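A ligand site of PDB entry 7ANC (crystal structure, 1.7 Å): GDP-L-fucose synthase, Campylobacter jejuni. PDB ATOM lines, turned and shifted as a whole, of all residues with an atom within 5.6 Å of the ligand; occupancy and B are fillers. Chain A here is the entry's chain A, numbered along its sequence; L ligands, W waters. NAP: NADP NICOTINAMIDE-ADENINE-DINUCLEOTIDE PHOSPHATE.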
ATOM      1  N   GLY A  12     -23.829   0.770  22.353  1.00  0.00           N
ATOM      2  CA  GLY A  12     -23.070  -0.468  22.464  1.00  0.00           C
ATOM      3  C   GLY A  12     -21.944  -0.448  23.474  1.00  0.00           C
ATOM      4  O   GLY A  12     -20.815  -0.931  23.232  1.00  0.00           O
ATOM      5  N   HIS A  13     -22.268   0.088  24.670  1.00  0.00           N
ATOM      6  CA  HIS A  13     -21.250   0.415  25.655  1.00  0.00           C
ATOM      7  C   HIS A  13     -20.572  -0.789  26.351  1.00  0.00           C
ATOM      8  O   HIS A  13     -19.544  -0.601  26.975  1.00  0.00           O
ATOM      9  CB  HIS A  13     -21.805   1.381  26.704  1.00  0.00           C
ATOM     10  CG  HIS A  13     -22.742   0.740  27.691  1.00  0.00           C
ATOM     11  ND1 HIS A  13     -24.069   0.472  27.395  1.00  0.00           N
ATOM     12  CD2 HIS A  13     -22.536   0.311  28.964  1.00  0.00           C
ATOM     13  CE1 HIS A  13     -24.630  -0.096  28.454  1.00  0.00           C
ATOM     14  NE2 HIS A  13     -23.730  -0.202  29.418  1.00  0.00           N
ATOM     15  N   LYS A  14     -21.137  -1.995  26.228  1.00  0.00           N
ATOM     16  CA  LYS A  14     -20.502  -3.218  26.806  1.00  0.00           C
ATOM     17  C   LYS A  14     -19.467  -3.948  25.945  1.00  0.00           C
ATOM     18  O   LYS A  14     -18.793  -4.845  26.418  1.00  0.00           O
ATOM     19  CB  LYS A  14     -21.571  -4.239  27.305  1.00  0.00           C
ATOM     20  CG  LYS A  14     -22.625  -3.650  28.229  1.00  0.00           C
ATOM     21  CD  LYS A  14     -22.180  -3.643  29.673  1.00  0.00           C
ATOM     22  CE  LYS A  14     -22.405  -5.009  30.291  1.00  0.00           C
ATOM     23  NZ  LYS A  14     -21.309  -5.313  31.244  1.00  0.00           N
ATOM     24  N   GLY A  15     -19.333  -3.550  24.678  1.00  0.00           N
ATOM     25  CA  GLY A  15     -18.347  -4.117  23.777  1.00  0.00           C
ATOM     26  C   GLY A  15     -16.927  -3.627  24.058  1.00  0.00           C
ATOM     27  O   GLY A  15     -16.723  -2.807  24.968  1.00  0.00           O
ATOM     28  N   THR A  16     -15.970  -4.085  23.253  1.00  0.00           N
ATOM     29  CA  THR A  16     -14.569  -3.698  23.397  1.00  0.00           C
ATOM     30  C   THR A  16     -14.326  -2.175  23.240  1.00  0.00           C
ATOM     31  O   THR A  16     -13.759  -1.536  24.116  1.00  0.00           O
ATOM     32  CB  THR A  16     -13.670  -4.481  22.450  1.00  0.00           C
ATOM     33  OG1 THR A  16     -13.838  -5.871  22.674  1.00  0.00           O
ATOM     34  CG2 THR A  16     -12.182  -4.125  22.664  1.00  0.00           C
ATOM     35  N   ALA A  17     -14.807  -1.613  22.125  1.00  0.00           N
ATOM     36  CA  ALA A  17     -14.691  -0.156  21.920  1.00  0.00           C
ATOM     37  C   ALA A  17     -15.514   0.655  22.898  1.00  0.00           C
ATOM     38  O   ALA A  17     -15.048   1.666  23.442  1.00  0.00           O
ATOM     39  CB  ALA A  17     -15.038   0.216  20.483  1.00  0.00           C
ATOM     40  N   GLY A  18     -16.763   0.238  23.107  1.00  0.00           N
ATOM     41  CA  GLY A  18     -17.642   0.879  24.056  1.00  0.00           C
ATOM     42  C   GLY A  18     -17.116   0.963  25.470  1.00  0.00           C
ATOM     43  O   GLY A  18     -17.196   2.032  26.107  1.00  0.00           O
ATOM     44  N   THR A  37     -28.236  -0.930  28.054  1.00  0.00           N
ATOM     45  CA  THR A  37     -27.944  -2.310  27.655  1.00  0.00           C
ATOM     46  C   THR A  37     -28.869  -2.719  26.492  1.00  0.00           C
ATOM     47  O   THR A  37     -29.879  -2.052  26.259  1.00  0.00           O
ATOM     48  CB  THR A  37     -28.170  -3.313  28.814  1.00  0.00           C
ATOM     49  OG1 THR A  37     -29.575  -3.351  29.138  1.00  0.00           O
ATOM     50  CG2 THR A  37     -27.322  -2.942  30.041  1.00  0.00           C
ATOM     51  N   ARG A  38     -28.490  -3.771  25.766  1.00  0.00           N
ATOM     52  CA  ARG A  38     -29.324  -4.381  24.737  1.00  0.00           C
ATOM     53  C   ARG A  38     -30.728  -4.711  25.222  1.00  0.00           C
ATOM     54  O   ARG A  38     -31.717  -4.492  24.521  1.00  0.00           O
ATOM     55  CB  ARG A  38     -28.659  -5.645  24.196  1.00  0.00           C
ATOM     56  CG  ARG A  38     -29.416  -6.221  23.001  1.00  0.00           C
ATOM     57  CD  ARG A  38     -29.067  -7.697  22.756  1.00  0.00           C
ATOM     58  NE  ARG A  38     -27.709  -7.880  22.222  1.00  0.00           N
ATOM     59  CZ  ARG A  38     -27.404  -7.987  20.924  1.00  0.00           C
ATOM     60  NH1 ARG A  38     -28.341  -7.900  19.976  1.00  0.00           N
ATOM     61  NH2 ARG A  38     -26.145  -8.196  20.555  1.00  0.00           N
ATOM     62  N   GLN A  39     -30.841  -5.211  26.457  1.00  0.00           N
ATOM     63  CA  GLN A  39     -32.151  -5.523  27.065  1.00  0.00           C
ATOM     64  C   GLN A  39     -33.009  -4.287  27.333  1.00  0.00           C
ATOM     65  O   GLN A  39     -34.220  -4.325  27.242  1.00  0.00           O
ATOM     66  CB  GLN A  39     -31.933  -6.341  28.365  1.00  0.00           C
ATOM     67  CG  GLN A  39     -31.272  -7.712  28.185  1.00  0.00           C
ATOM     68  CD  GLN A  39     -29.798  -7.709  27.788  1.00  0.00           C
ATOM     69  OE1 GLN A  39     -29.004  -6.827  28.186  1.00  0.00           O
ATOM     70  NE2 GLN A  39     -29.409  -8.711  26.977  1.00  0.00           N
ATOM     71  N   LEU A  41     -32.669  -1.404  25.426  1.00  0.00           N
ATOM     72  CA  LEU A  41     -32.863  -0.701  24.158  1.00  0.00           C
ATOM     73  C   LEU A  41     -32.288  -1.525  23.001  1.00  0.00           C
ATOM     74  O   LEU A  41     -31.074  -1.673  22.892  1.00  0.00           O
ATOM     75  CB  LEU A  41     -32.233   0.707  24.213  1.00  0.00           C
ATOM     76  CG  LEU A  41     -32.196   1.561  22.923  1.00  0.00           C
ATOM     77  CD1 LEU A  41     -33.612   1.808  22.401  1.00  0.00           C
ATOM     78  CD2 LEU A  41     -31.476   2.901  23.156  1.00  0.00           C
ATOM     79  N   ASP A  42     -33.182  -2.106  22.193  1.00  0.00           N
ATOM     80  CA  ASP A  42     -32.791  -2.862  21.007  1.00  0.00           C
ATOM     81  C   ASP A  42     -32.586  -1.891  19.834  1.00  0.00           C
ATOM     82  O   ASP A  42     -33.546  -1.313  19.354  1.00  0.00           O
ATOM     83  CB  ASP A  42     -33.897  -3.881  20.639  1.00  0.00           C
ATOM     84  CG  ASP A  42     -33.581  -4.655  19.372  1.00  0.00           C
ATOM     85  OD1 ASP A  42     -32.458  -4.517  18.792  1.00  0.00           O
ATOM     86  OD2 ASP A  42     -34.488  -5.414  18.964  1.00  0.00           O
ATOM     87  N   LEU A  43     -31.332  -1.697  19.420  1.00  0.00           N
ATOM     88  CA  LEU A  43     -31.016  -0.644  18.425  1.00  0.00           C
ATOM     89  C   LEU A  43     -31.528  -0.978  17.000  1.00  0.00           C
ATOM     90  O   LEU A  43     -31.518  -0.108  16.148  1.00  0.00           O
ATOM     91  CB  LEU A  43     -29.519  -0.330  18.410  1.00  0.00           C
ATOM     92  CG  LEU A  43     -29.022   0.327  19.719  1.00  0.00           C
ATOM     93  CD1 LEU A  43     -27.483   0.348  19.710  1.00  0.00           C
ATOM     94  CD2 LEU A  43     -29.573   1.709  19.886  1.00  0.00           C
ATOM     95  N   VAL A  44     -31.968  -2.215  16.771  1.00  0.00           N
ATOM     96  CA  VAL A  44     -32.636  -2.614  15.517  1.00  0.00           C
ATOM     97  C   VAL A  44     -34.106  -2.110  15.429  1.00  0.00           C
ATOM     98  O   VAL A  44     -34.676  -1.949  14.351  1.00  0.00           O
ATOM     99  CB  VAL A  44     -32.491  -4.153  15.302  1.00  0.00           C
ATOM    100  CG1 VAL A  44     -33.308  -4.621  14.097  1.00  0.00           C
ATOM    101  CG2 VAL A  44     -31.029  -4.526  15.132  1.00  0.00           C
ATOM    102  N   LEU A  63     -21.121   5.897  18.139  1.00  0.00           N
ATOM    103  CA  LEU A  63     -21.833   4.721  17.640  1.00  0.00           C
ATOM    104  C   LEU A  63     -20.865   3.522  17.527  1.00  0.00           C
ATOM    105  O   LEU A  63     -20.196   3.375  16.509  1.00  0.00           O
ATOM    106  CB  LEU A  63     -22.552   5.072  16.330  1.00  0.00           C
ATOM    107  CG  LEU A  63     -23.319   3.929  15.663  1.00  0.00           C
ATOM    108  CD1 LEU A  63     -24.267   3.221  16.630  1.00  0.00           C
ATOM    109  CD2 LEU A  63     -24.050   4.440  14.456  1.00  0.00           C
ATOM    110  N   THR A  64     -20.799   2.701  18.570  1.00  0.00           N
ATOM    111  CA  THR A  64     -19.941   1.493  18.570  1.00  0.00           C
ATOM    112  C   THR A  64     -20.659   0.148  18.396  1.00  0.00           C
ATOM    113  O   THR A  64     -20.005  -0.837  18.111  1.00  0.00           O
ATOM    114  CB  THR A  64     -19.032   1.389  19.837  1.00  0.00           C
ATOM    115  OG1 THR A  64     -19.780   0.889  20.960  1.00  0.00           O
ATOM    116  CG2 THR A  64     -18.468   2.713  20.206  1.00  0.00           C
ATOM    117  N   ALA A  65     -21.996   0.126  18.497  1.00  0.00           N
ATOM    118  CA  ALA A  65     -22.779  -1.113  18.449  1.00  0.00           C
ATOM    119  C   ALA A  65     -22.682  -1.761  17.052  1.00  0.00           C
ATOM    120  O   ALA A  65     -22.783  -1.063  16.044  1.00  0.00           O
ATOM    121  CB  ALA A  65     -24.238  -0.800  18.774  1.00  0.00           C
ATOM    122  N   VAL A  66     -22.517  -3.086  17.019  1.00  0.00           N
ATOM    123  CA  VAL A  66     -22.340  -3.846  15.779  1.00  0.00           C
ATOM    124  C   VAL A  66     -22.668  -5.323  16.040  1.00  0.00           C
ATOM    125  O   VAL A  66     -22.525  -5.817  17.175  1.00  0.00           O
ATOM    126  CB  VAL A  66     -20.886  -3.723  15.267  1.00  0.00           C
ATOM    127  CG1 VAL A  66     -19.901  -4.540  16.103  1.00  0.00           C
ATOM    128  CG2 VAL A  66     -20.733  -4.142  13.812  1.00  0.00           C
ATOM    129  N   LEU A  67     -23.145  -5.998  14.987  1.00  0.00           N
ATOM    130  CA  LEU A  67     -23.048  -7.452  14.872  1.00  0.00           C
ATOM    131  C   LEU A  67     -21.786  -7.760  14.066  1.00  0.00           C
ATOM    132  O   LEU A  67     -21.762  -7.571  12.844  1.00  0.00           O
ATOM    133  CB  LEU A  67     -24.297  -8.043  14.184  1.00  0.00           C
ATOM    134  CG  LEU A  67     -24.182  -9.575  13.925  1.00  0.00           C
ATOM    135  CD1 LEU A  67     -24.124 -10.333  15.264  1.00  0.00           C
ATOM    136  CD2 LEU A  67     -25.349 -10.043  13.070  1.00  0.00           C
ATOM    137  N   PRO A  68     -20.688  -8.222  14.714  1.00  0.00           N
ATOM    138  CA  PRO A  68     -19.413  -8.382  14.024  1.00  0.00           C
ATOM    139  C   PRO A  68     -19.325  -9.701  13.286  1.00  0.00           C
ATOM    140  O   PRO A  68     -19.939 -10.691  13.719  1.00  0.00           O
ATOM    141  CB  PRO A  68     -18.400  -8.376  15.184  1.00  0.00           C
ATOM    142  CG  PRO A  68     -19.159  -8.997  16.314  1.00  0.00           C
ATOM    143  CD  PRO A  68     -20.607  -8.594  16.149  1.00  0.00           C
ATOM    144  N   GLU A  83     -28.963  -6.251  10.214  1.00  0.00           N
ATOM    145  CA  GLU A  83     -28.818  -5.685  11.569  1.00  0.00           C
ATOM    146  C   GLU A  83     -27.954  -4.432  11.619  1.00  0.00           C
ATOM    147  O   GLU A  83     -28.331  -3.423  12.232  1.00  0.00           O
ATOM    148  CB  GLU A  83     -28.373  -6.764  12.579  1.00  0.00           C
ATOM    149  CG  GLU A  83     -29.420  -7.865  12.696  1.00  0.00           C
ATOM    150  CD  GLU A  83     -29.136  -8.897  13.787  1.00  0.00           C
ATOM    151  OE1 GLU A  83     -28.367  -8.577  14.748  1.00  0.00           O
ATOM    152  OE2 GLU A  83     -29.665 -10.029  13.666  1.00  0.00           O
ATOM    153  N   ILE A  87     -29.186  -0.593  12.709  1.00  0.00           N
ATOM    154  CA  ILE A  87     -28.515   0.099  13.824  1.00  0.00           C
ATOM    155  C   ILE A  87     -28.024   1.481  13.314  1.00  0.00           C
ATOM    156  O   ILE A  87     -28.305   2.559  13.921  1.00  0.00           O
ATOM    157  CB  ILE A  87     -27.339  -0.734  14.376  1.00  0.00           C
ATOM    158  CG1 ILE A  87     -27.871  -1.968  15.090  1.00  0.00           C
ATOM    159  CG2 ILE A  87     -26.442   0.074  15.329  1.00  0.00           C
ATOM    160  CD1 ILE A  87     -26.805  -2.972  15.441  1.00  0.00           C
ATOM    161  N   PHE A 105     -18.848   7.553  14.040  1.00  0.00           N
ATOM    162  CA  PHE A 105     -19.231   6.201  13.600  1.00  0.00           C
ATOM    163  C   PHE A 105     -17.932   5.443  13.244  1.00  0.00           C
ATOM    164  O   PHE A 105     -17.003   6.047  12.719  1.00  0.00           O
ATOM    165  CB  PHE A 105     -20.142   6.287  12.365  1.00  0.00           C
ATOM    166  CG  PHE A 105     -20.394   4.964  11.662  1.00  0.00           C
ATOM    167  CD1 PHE A 105     -20.997   3.900  12.335  1.00  0.00           C
ATOM    168  CD2 PHE A 105     -20.008   4.778  10.334  1.00  0.00           C
ATOM    169  CE1 PHE A 105     -21.201   2.660  11.695  1.00  0.00           C
ATOM    170  CE2 PHE A 105     -20.213   3.574   9.699  1.00  0.00           C
ATOM    171  CZ  PHE A 105     -20.833   2.504  10.389  1.00  0.00           C
ATOM    172  N   PHE A 106     -17.880   4.139  13.525  1.00  0.00           N
ATOM    173  CA  PHE A 106     -16.703   3.283  13.239  1.00  0.00           C
ATOM    174  C   PHE A 106     -16.915   2.357  12.043  1.00  0.00           C
ATOM    175  O   PHE A 106     -17.834   1.512  12.066  1.00  0.00           O
ATOM    176  CB  PHE A 106     -16.272   2.501  14.496  1.00  0.00           C
ATOM    177  CG  PHE A 106     -15.871   3.382  15.650  1.00  0.00           C
ATOM    178  CD1 PHE A 106     -14.594   3.945  15.691  1.00  0.00           C
ATOM    179  CD2 PHE A 106     -16.764   3.734  16.635  1.00  0.00           C
ATOM    180  CE1 PHE A 106     -14.215   4.772  16.717  1.00  0.00           C
ATOM    181  CE2 PHE A 106     -16.391   4.610  17.648  1.00  0.00           C
ATOM    182  CZ  PHE A 106     -15.117   5.101  17.703  1.00  0.00           C
ATOM    183  N   GLY A 107     -16.086   2.521  11.011  1.00  0.00           N
ATOM    184  CA  GLY A 107     -16.025   1.644   9.872  1.00  0.00           C
ATOM    185  C   GLY A 107     -14.956   0.543  10.045  1.00  0.00           C
ATOM    186  O   GLY A 107     -14.203   0.529  11.018  1.00  0.00           O
ATOM    187  N   SER A 108     -14.911  -0.368   9.073  1.00  0.00           N
ATOM    188  CA  SER A 108     -13.990  -1.522   9.047  1.00  0.00           C
ATOM    189  C   SER A 108     -13.225  -1.552   7.726  1.00  0.00           C
ATOM    190  O   SER A 108     -13.790  -1.234   6.669  1.00  0.00           O
ATOM    191  CB  SER A 108     -14.775  -2.848   9.168  1.00  0.00           C
ATOM    192  OG  SER A 108     -13.952  -3.977   8.806  1.00  0.00           O
ATOM    193  N   GLY A 109     -11.960  -2.012   7.768  1.00  0.00           N
ATOM    194  CA  GLY A 109     -11.152  -2.193   6.563  1.00  0.00           C
ATOM    195  C   GLY A 109     -11.709  -3.206   5.558  1.00  0.00           C
ATOM    196  O   GLY A 109     -11.262  -3.241   4.382  1.00  0.00           O
ATOM    197  N   PHE A 137     -21.131  -7.707   5.262  1.00  0.00           N
ATOM    198  CA  PHE A 137     -20.679  -6.832   6.365  1.00  0.00           C
ATOM    199  C   PHE A 137     -19.973  -5.579   5.817  1.00  0.00           C
ATOM    200  O   PHE A 137     -20.270  -4.428   6.209  1.00  0.00           O
ATOM    201  CB  PHE A 137     -19.742  -7.630   7.278  1.00  0.00           C
ATOM    202  CG  PHE A 137     -19.146  -6.818   8.412  1.00  0.00           C
ATOM    203  CD1 PHE A 137     -19.859  -6.612   9.590  1.00  0.00           C
ATOM    204  CD2 PHE A 137     -17.888  -6.290   8.292  1.00  0.00           C
ATOM    205  CE1 PHE A 137     -19.319  -5.865  10.630  1.00  0.00           C
ATOM    206  CE2 PHE A 137     -17.327  -5.523   9.342  1.00  0.00           C
ATOM    207  CZ  PHE A 137     -18.041  -5.335  10.506  1.00  0.00           C
ATOM    208  N   LYS A 141     -21.065  -1.498   6.036  1.00  0.00           N
ATOM    209  CA  LYS A 141     -20.119  -0.454   6.486  1.00  0.00           C
ATOM    210  C   LYS A 141     -19.923   0.671   5.473  1.00  0.00           C
ATOM    211  O   LYS A 141     -19.877   1.841   5.857  1.00  0.00           O
ATOM    212  CB  LYS A 141     -18.780  -1.038   6.964  1.00  0.00           C
ATOM    213  CG  LYS A 141     -18.885  -1.868   8.231  1.00  0.00           C
ATOM    214  CD  LYS A 141     -19.367  -1.060   9.439  1.00  0.00           C
ATOM    215  CE  LYS A 141     -18.955  -1.723  10.742  1.00  0.00           C
ATOM    216  NZ  LYS A 141     -19.289  -0.873  11.939  1.00  0.00           N
ATOM    217  N   LEU A 164     -11.077   1.414  10.915  1.00  0.00           N
ATOM    218  CA  LEU A 164      -9.963   0.634  11.484  1.00  0.00           C
ATOM    219  C   LEU A 164      -9.953  -0.817  11.031  1.00  0.00           C
ATOM    220  O   LEU A 164     -10.962  -1.327  10.501  1.00  0.00           O
ATOM    221  CB  LEU A 164      -9.980   0.686  13.036  1.00  0.00           C
ATOM    222  CG  LEU A 164     -11.228   0.032  13.683  1.00  0.00           C
ATOM    223  CD1 LEU A 164     -10.825  -0.720  14.965  1.00  0.00           C
ATOM    224  CD2 LEU A 164     -12.347   1.009  13.944  1.00  0.00           C
ATOM    225  N   ASN A 165      -8.819  -1.506  11.267  1.00  0.00           N
ATOM    226  CA  ASN A 165      -8.679  -2.933  10.962  1.00  0.00           C
ATOM    227  C   ASN A 165      -8.895  -3.962  12.110  1.00  0.00           C
ATOM    228  O   ASN A 165      -9.828  -4.749  12.026  1.00  0.00           O
ATOM    229  CB  ASN A 165      -7.345  -3.210  10.219  1.00  0.00           C
ATOM    230  CG  ASN A 165      -7.370  -2.668   8.769  1.00  0.00           C
ATOM    231  OD1 ASN A 165      -8.328  -2.944   8.055  1.00  0.00           O
ATOM    232  ND2 ASN A 165      -6.346  -1.951   8.352  1.00  0.00           N
ATOM    233  N   ASN A 166      -7.949  -4.115  13.033  1.00  0.00           N
ATOM    234  CA  ASN A 166      -8.106  -5.100  14.183  1.00  0.00           C
ATOM    235  C   ASN A 166      -7.944  -4.381  15.526  1.00  0.00           C
ATOM    236  O   ASN A 166      -6.913  -3.773  15.787  1.00  0.00           O
ATOM    237  CB  ASN A 166      -7.100  -6.257  14.123  1.00  0.00           C
ATOM    238  CG  ASN A 166      -7.338  -7.176  12.951  1.00  0.00           C
ATOM    239  OD1 ASN A 166      -8.127  -8.107  13.031  1.00  0.00           O
ATOM    240  ND2 ASN A 166      -6.673  -6.901  11.854  1.00  0.00           N
ATOM    241  N   LEU A 167      -8.957  -4.501  16.362  1.00  0.00           N
ATOM    242  CA  LEU A 167      -8.976  -3.878  17.680  1.00  0.00           C
ATOM    243  C   LEU A 167      -8.614  -4.932  18.748  1.00  0.00           C
ATOM    244  O   LEU A 167      -9.070  -6.072  18.631  1.00  0.00           O
ATOM    245  CB  LEU A 167     -10.388  -3.374  17.945  1.00  0.00           C
ATOM    246  CG  LEU A 167     -10.657  -2.602  19.240  1.00  0.00           C
ATOM    247  CD1 LEU A 167      -9.837  -1.311  19.289  1.00  0.00           C
ATOM    248  CD2 LEU A 167     -12.145  -2.316  19.356  1.00  0.00           C
ATOM    249  N   LEU A 247      -7.846   3.750  20.315  1.00  0.00           N
ATOM    250  CA  LEU A 247      -9.133   3.976  19.659  1.00  0.00           C
ATOM    251  C   LEU A 247      -9.970   5.039  20.398  1.00  0.00           C
ATOM    252  O   LEU A 247     -10.481   5.983  19.784  1.00  0.00           O
ATOM    253  CB  LEU A 247      -9.939   2.642  19.515  1.00  0.00           C
ATOM    254  CG  LEU A 247     -11.322   2.809  18.815  1.00  0.00           C
ATOM    255  CD1 LEU A 247     -11.193   3.494  17.470  1.00  0.00           C
ATOM    256  CD2 LEU A 247     -12.066   1.534  18.540  1.00  0.00           C
HETATM  257  PA  NAP L   1     -18.160  -5.724  20.154  1.00  0.00           P
HETATM  258  O1A NAP L   1     -18.665  -6.874  19.314  1.00  0.00           O
HETATM  259  O2A NAP L   1     -17.076  -5.962  21.178  1.00  0.00           O
HETATM  260  O5B NAP L   1     -19.423  -5.016  20.836  1.00  0.00           O
HETATM  261  C5B NAP L   1     -20.670  -4.773  20.131  1.00  0.00           C
HETATM  262  C4B NAP L   1     -21.678  -4.222  21.124  1.00  0.00           C
HETATM  263  O4B NAP L   1     -22.869  -3.800  20.398  1.00  0.00           O
HETATM  264  C3B NAP L   1     -22.154  -5.227  22.200  1.00  0.00           C
HETATM  265  O3B NAP L   1     -22.162  -4.654  23.507  1.00  0.00           O
HETATM  266  C2B NAP L   1     -23.583  -5.537  21.783  1.00  0.00           C
HETATM  267  O2B NAP L   1     -24.428  -5.712  22.937  1.00  0.00           O
HETATM  268  C1B NAP L   1     -24.012  -4.237  21.088  1.00  0.00           C
HETATM  269  N9A NAP L   1     -25.163  -4.412  20.206  1.00  0.00           N
HETATM  270  C8A NAP L   1     -25.239  -5.195  19.075  1.00  0.00           C
HETATM  271  N7A NAP L   1     -26.442  -5.242  18.544  1.00  0.00           N
HETATM  272  C5A NAP L   1     -27.238  -4.469  19.390  1.00  0.00           C
HETATM  273  C6A NAP L   1     -28.609  -4.143  19.388  1.00  0.00           C
HETATM  274  N6A NAP L   1     -29.496  -4.628  18.496  1.00  0.00           N
HETATM  275  N1A NAP L   1     -29.082  -3.386  20.417  1.00  0.00           N
HETATM  276  C2A NAP L   1     -28.198  -2.933  21.336  1.00  0.00           C
HETATM  277  N3A NAP L   1     -26.888  -3.157  21.432  1.00  0.00           N
HETATM  278  C4A NAP L   1     -26.456  -3.962  20.434  1.00  0.00           C
HETATM  279  O3  NAP L   1     -17.655  -4.556  19.173  1.00  0.00           O
HETATM  280  PN  NAP L   1     -16.241  -3.816  19.090  1.00  0.00           P
HETATM  281  O1N NAP L   1     -16.062  -2.905  20.219  1.00  0.00           O
HETATM  282  O2N NAP L   1     -15.182  -4.828  18.777  1.00  0.00           O
HETATM  283  O5D NAP L   1     -16.454  -2.907  17.743  1.00  0.00           O
HETATM  284  C5D NAP L   1     -16.871  -1.520  17.921  1.00  0.00           C
HETATM  285  C4D NAP L   1     -16.936  -0.888  16.555  1.00  0.00           C
HETATM  286  O4D NAP L   1     -15.613  -1.015  15.965  1.00  0.00           O
HETATM  287  C3D NAP L   1     -17.919  -1.553  15.578  1.00  0.00           C
HETATM  288  O3D NAP L   1     -18.548  -0.609  14.723  1.00  0.00           O
HETATM  289  C2D NAP L   1     -16.983  -2.515  14.806  1.00  0.00           C
HETATM  290  O2D NAP L   1     -17.434  -2.922  13.510  1.00  0.00           O
HETATM  291  C1D NAP L   1     -15.735  -1.629  14.710  1.00  0.00           C
HETATM  292  N1N NAP L   1     -14.502  -2.410  14.422  1.00  0.00           N
HETATM  293  C2N NAP L   1     -13.964  -3.244  15.372  1.00  0.00           C
HETATM  294  C3N NAP L   1     -13.028  -4.179  15.028  1.00  0.00           C
HETATM  295  C7N NAP L   1     -12.626  -5.219  15.992  1.00  0.00           C
HETATM  296  O7N NAP L   1     -13.274  -5.474  17.030  1.00  0.00           O
HETATM  297  N7N NAP L   1     -11.499  -5.836  15.637  1.00  0.00           N
HETATM  298  C4N NAP L   1     -12.389  -4.101  13.673  1.00  0.00           C
HETATM  299  C5N NAP L   1     -13.033  -3.175  12.738  1.00  0.00           C
HETATM  300  C6N NAP L   1     -13.929  -2.311  13.157  1.00  0.00           C
HETATM  301  P2B NAP L   1     -24.289  -7.132  23.785  1.00  0.00           P
HETATM  302  O1X NAP L   1     -23.025  -6.990  24.654  1.00  0.00           O
HETATM  303  O2X NAP L   1     -25.589  -7.154  24.595  1.00  0.00           O
HETATM  304  O3X NAP L   1     -24.196  -8.295  22.809  1.00  0.00           O
HETATM  305  O   HOH W   1     -23.870  -2.967  25.180  1.00  0.00           O
HETATM  306  O   HOH W   2     -14.395  -7.990  15.590  1.00  0.00           O
HETATM  307  O   HOH W   3     -25.715  -4.946  26.234  1.00  0.00           O
HETATM  308  O   HOH W   4     -28.711  -0.529  23.675  1.00  0.00           O
HETATM  309  O   HOH W   5     -27.896  -6.704  16.609  1.00  0.00           O
HETATM  310  O   HOH W   6     -11.936  -5.140  10.252  1.00  0.00           O
HETATM  311  O   HOH W   7     -20.751  -8.496  19.886  1.00  0.00           O
HETATM  312  O   HOH W   8     -21.245   0.627  14.890  1.00  0.00           O
HETATM  313  O   HOH W   9     -18.341  -1.668  21.735  1.00  0.00           O
HETATM  314  O   HOH W  10     -25.686  -1.609  23.885  1.00  0.00           O
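O2A of the ligand is in hydrogen-bond range of N of Thr 16 (3.0 Å). O of Phe 106 is in hydrogen-bond range of O3D of the ligand, 3.5 Å away. O3D of the ligand is in hydrogen-bond range of NZ of Lys 141. N1A of the ligand lies within hydrogen-bond range of N of Leu 43, at 3.0 Å. An oxygen (O3X) of the ligand is in salt-bridge range of the guanidinium group (NH2) of Arg 38. An oxygen (O4B) of the ligand lies within hydrogen-bond range of the backbone NH (N) of Val 66 (3.5 Å). O3B of the ligand lies within hydrogen-bond range of N of Gly 15 (3.3 Å). A nitrogen (N6A) of the ligand lies within hydrogen-bond range of the side-chain carboxylate (OD1) of Asp 42, at 3.0 Å. N of Ala 17 lies within hydrogen-bond range of O1N of the ligand (2.6 Å).
The backbone carbonyl oxygen (O) of Gly 107 lies within hydrogen-bond range of the backbone NH (N) of Leu 164, 3.3 Å away. OG1 of Thr 64 sits at hydrogen-bond distance from O of Gly 12 (3.1 Å). OD1 of Asp 42 sits at hydrogen-bond distance from N of Val 44, 3.1 Å away. O of Leu 164 sits at hydrogen-bond distance from N of Gly 109. O of Phe 106 lies within hydrogen-bond range of NZ of Lys 141, 2.8 Å away.
The backbone NH (N) of Leu 167 lies close to a nitrogen (N7N) of the ligand, at 3.0 Å. CA of Gly 12 touches O4B of the ligand, at 3.9 Å. Lys 14 touches the ligand (C to O3B, 3.7 Å). Leu 41 touches the ligand. CG2 of Val 44 touches N6A of the ligand, 3.7 Å away. Thr 64 touches the ligand. Ala 65 touches the ligand (CA to O4B, 3.3 Å). Pro 68 touches the ligand (CG to O1A, 3.7 Å). CD1 of Ile 87 touches N7A of the ligand (3.9 Å). Gly 107 touches the ligand. Ser 108 touches the ligand (CB to C5N, 3.99 Å). CZ of Phe 137 touches O2D of the ligand, 3.9 Å away. O of Leu 164 touches C5N of the ligand, at 3.6 Å. Asn 165 touches the ligand. Asn 166 touches the ligand. Hydrophobic or aromatic side chains within 4 Å of the ligand: Ala 17, Leu 43, Val 44, Ala 65, Val 66, Pro 68, Ile 87, Phe 106, Phe 137, Leu 164 and Leu 167. Of the 34 residues printed, 24 come within 4 Å of the ligand.
Water W3 lies within hydrogen-bond range of an oxygen (O2X) of the ligand (2.8 Å) and the backbone NH (N) of Arg 38 (3.0 Å). Water W5 lies within hydrogen-bond range of the side-chain carboxylate (OE1) of Glu 83 (2.7 Å) and a nitrogen (N7A) of the ligand (2.8 Å). Water W1 lies within hydrogen-bond range of an oxygen (O3B) of the ligand (2.9 Å), the backbone NH of Lys 14 (3.1 Å) and the backbone NH of His 13 (3.5 Å). Water W8 lies within hydrogen-bond range of the backbone carbonyl oxygen (O) of Ala 65, an oxygen (O3D) of the ligand and the backbone carbonyl oxygen (O) of Leu 63. Water W9 lies within hydrogen-bond range of N of Gly 18 (2.8 Å), O of Gly 12 (3.0 Å), O1N of the ligand (3.0 Å) and OG1 of Thr 64 (3.0 Å). Water W6 bridges the side-chain hydroxyl of Ser 108 (2.7 Å) and the backbone carbonyl oxygen of Asn 165 (2.8 Å).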
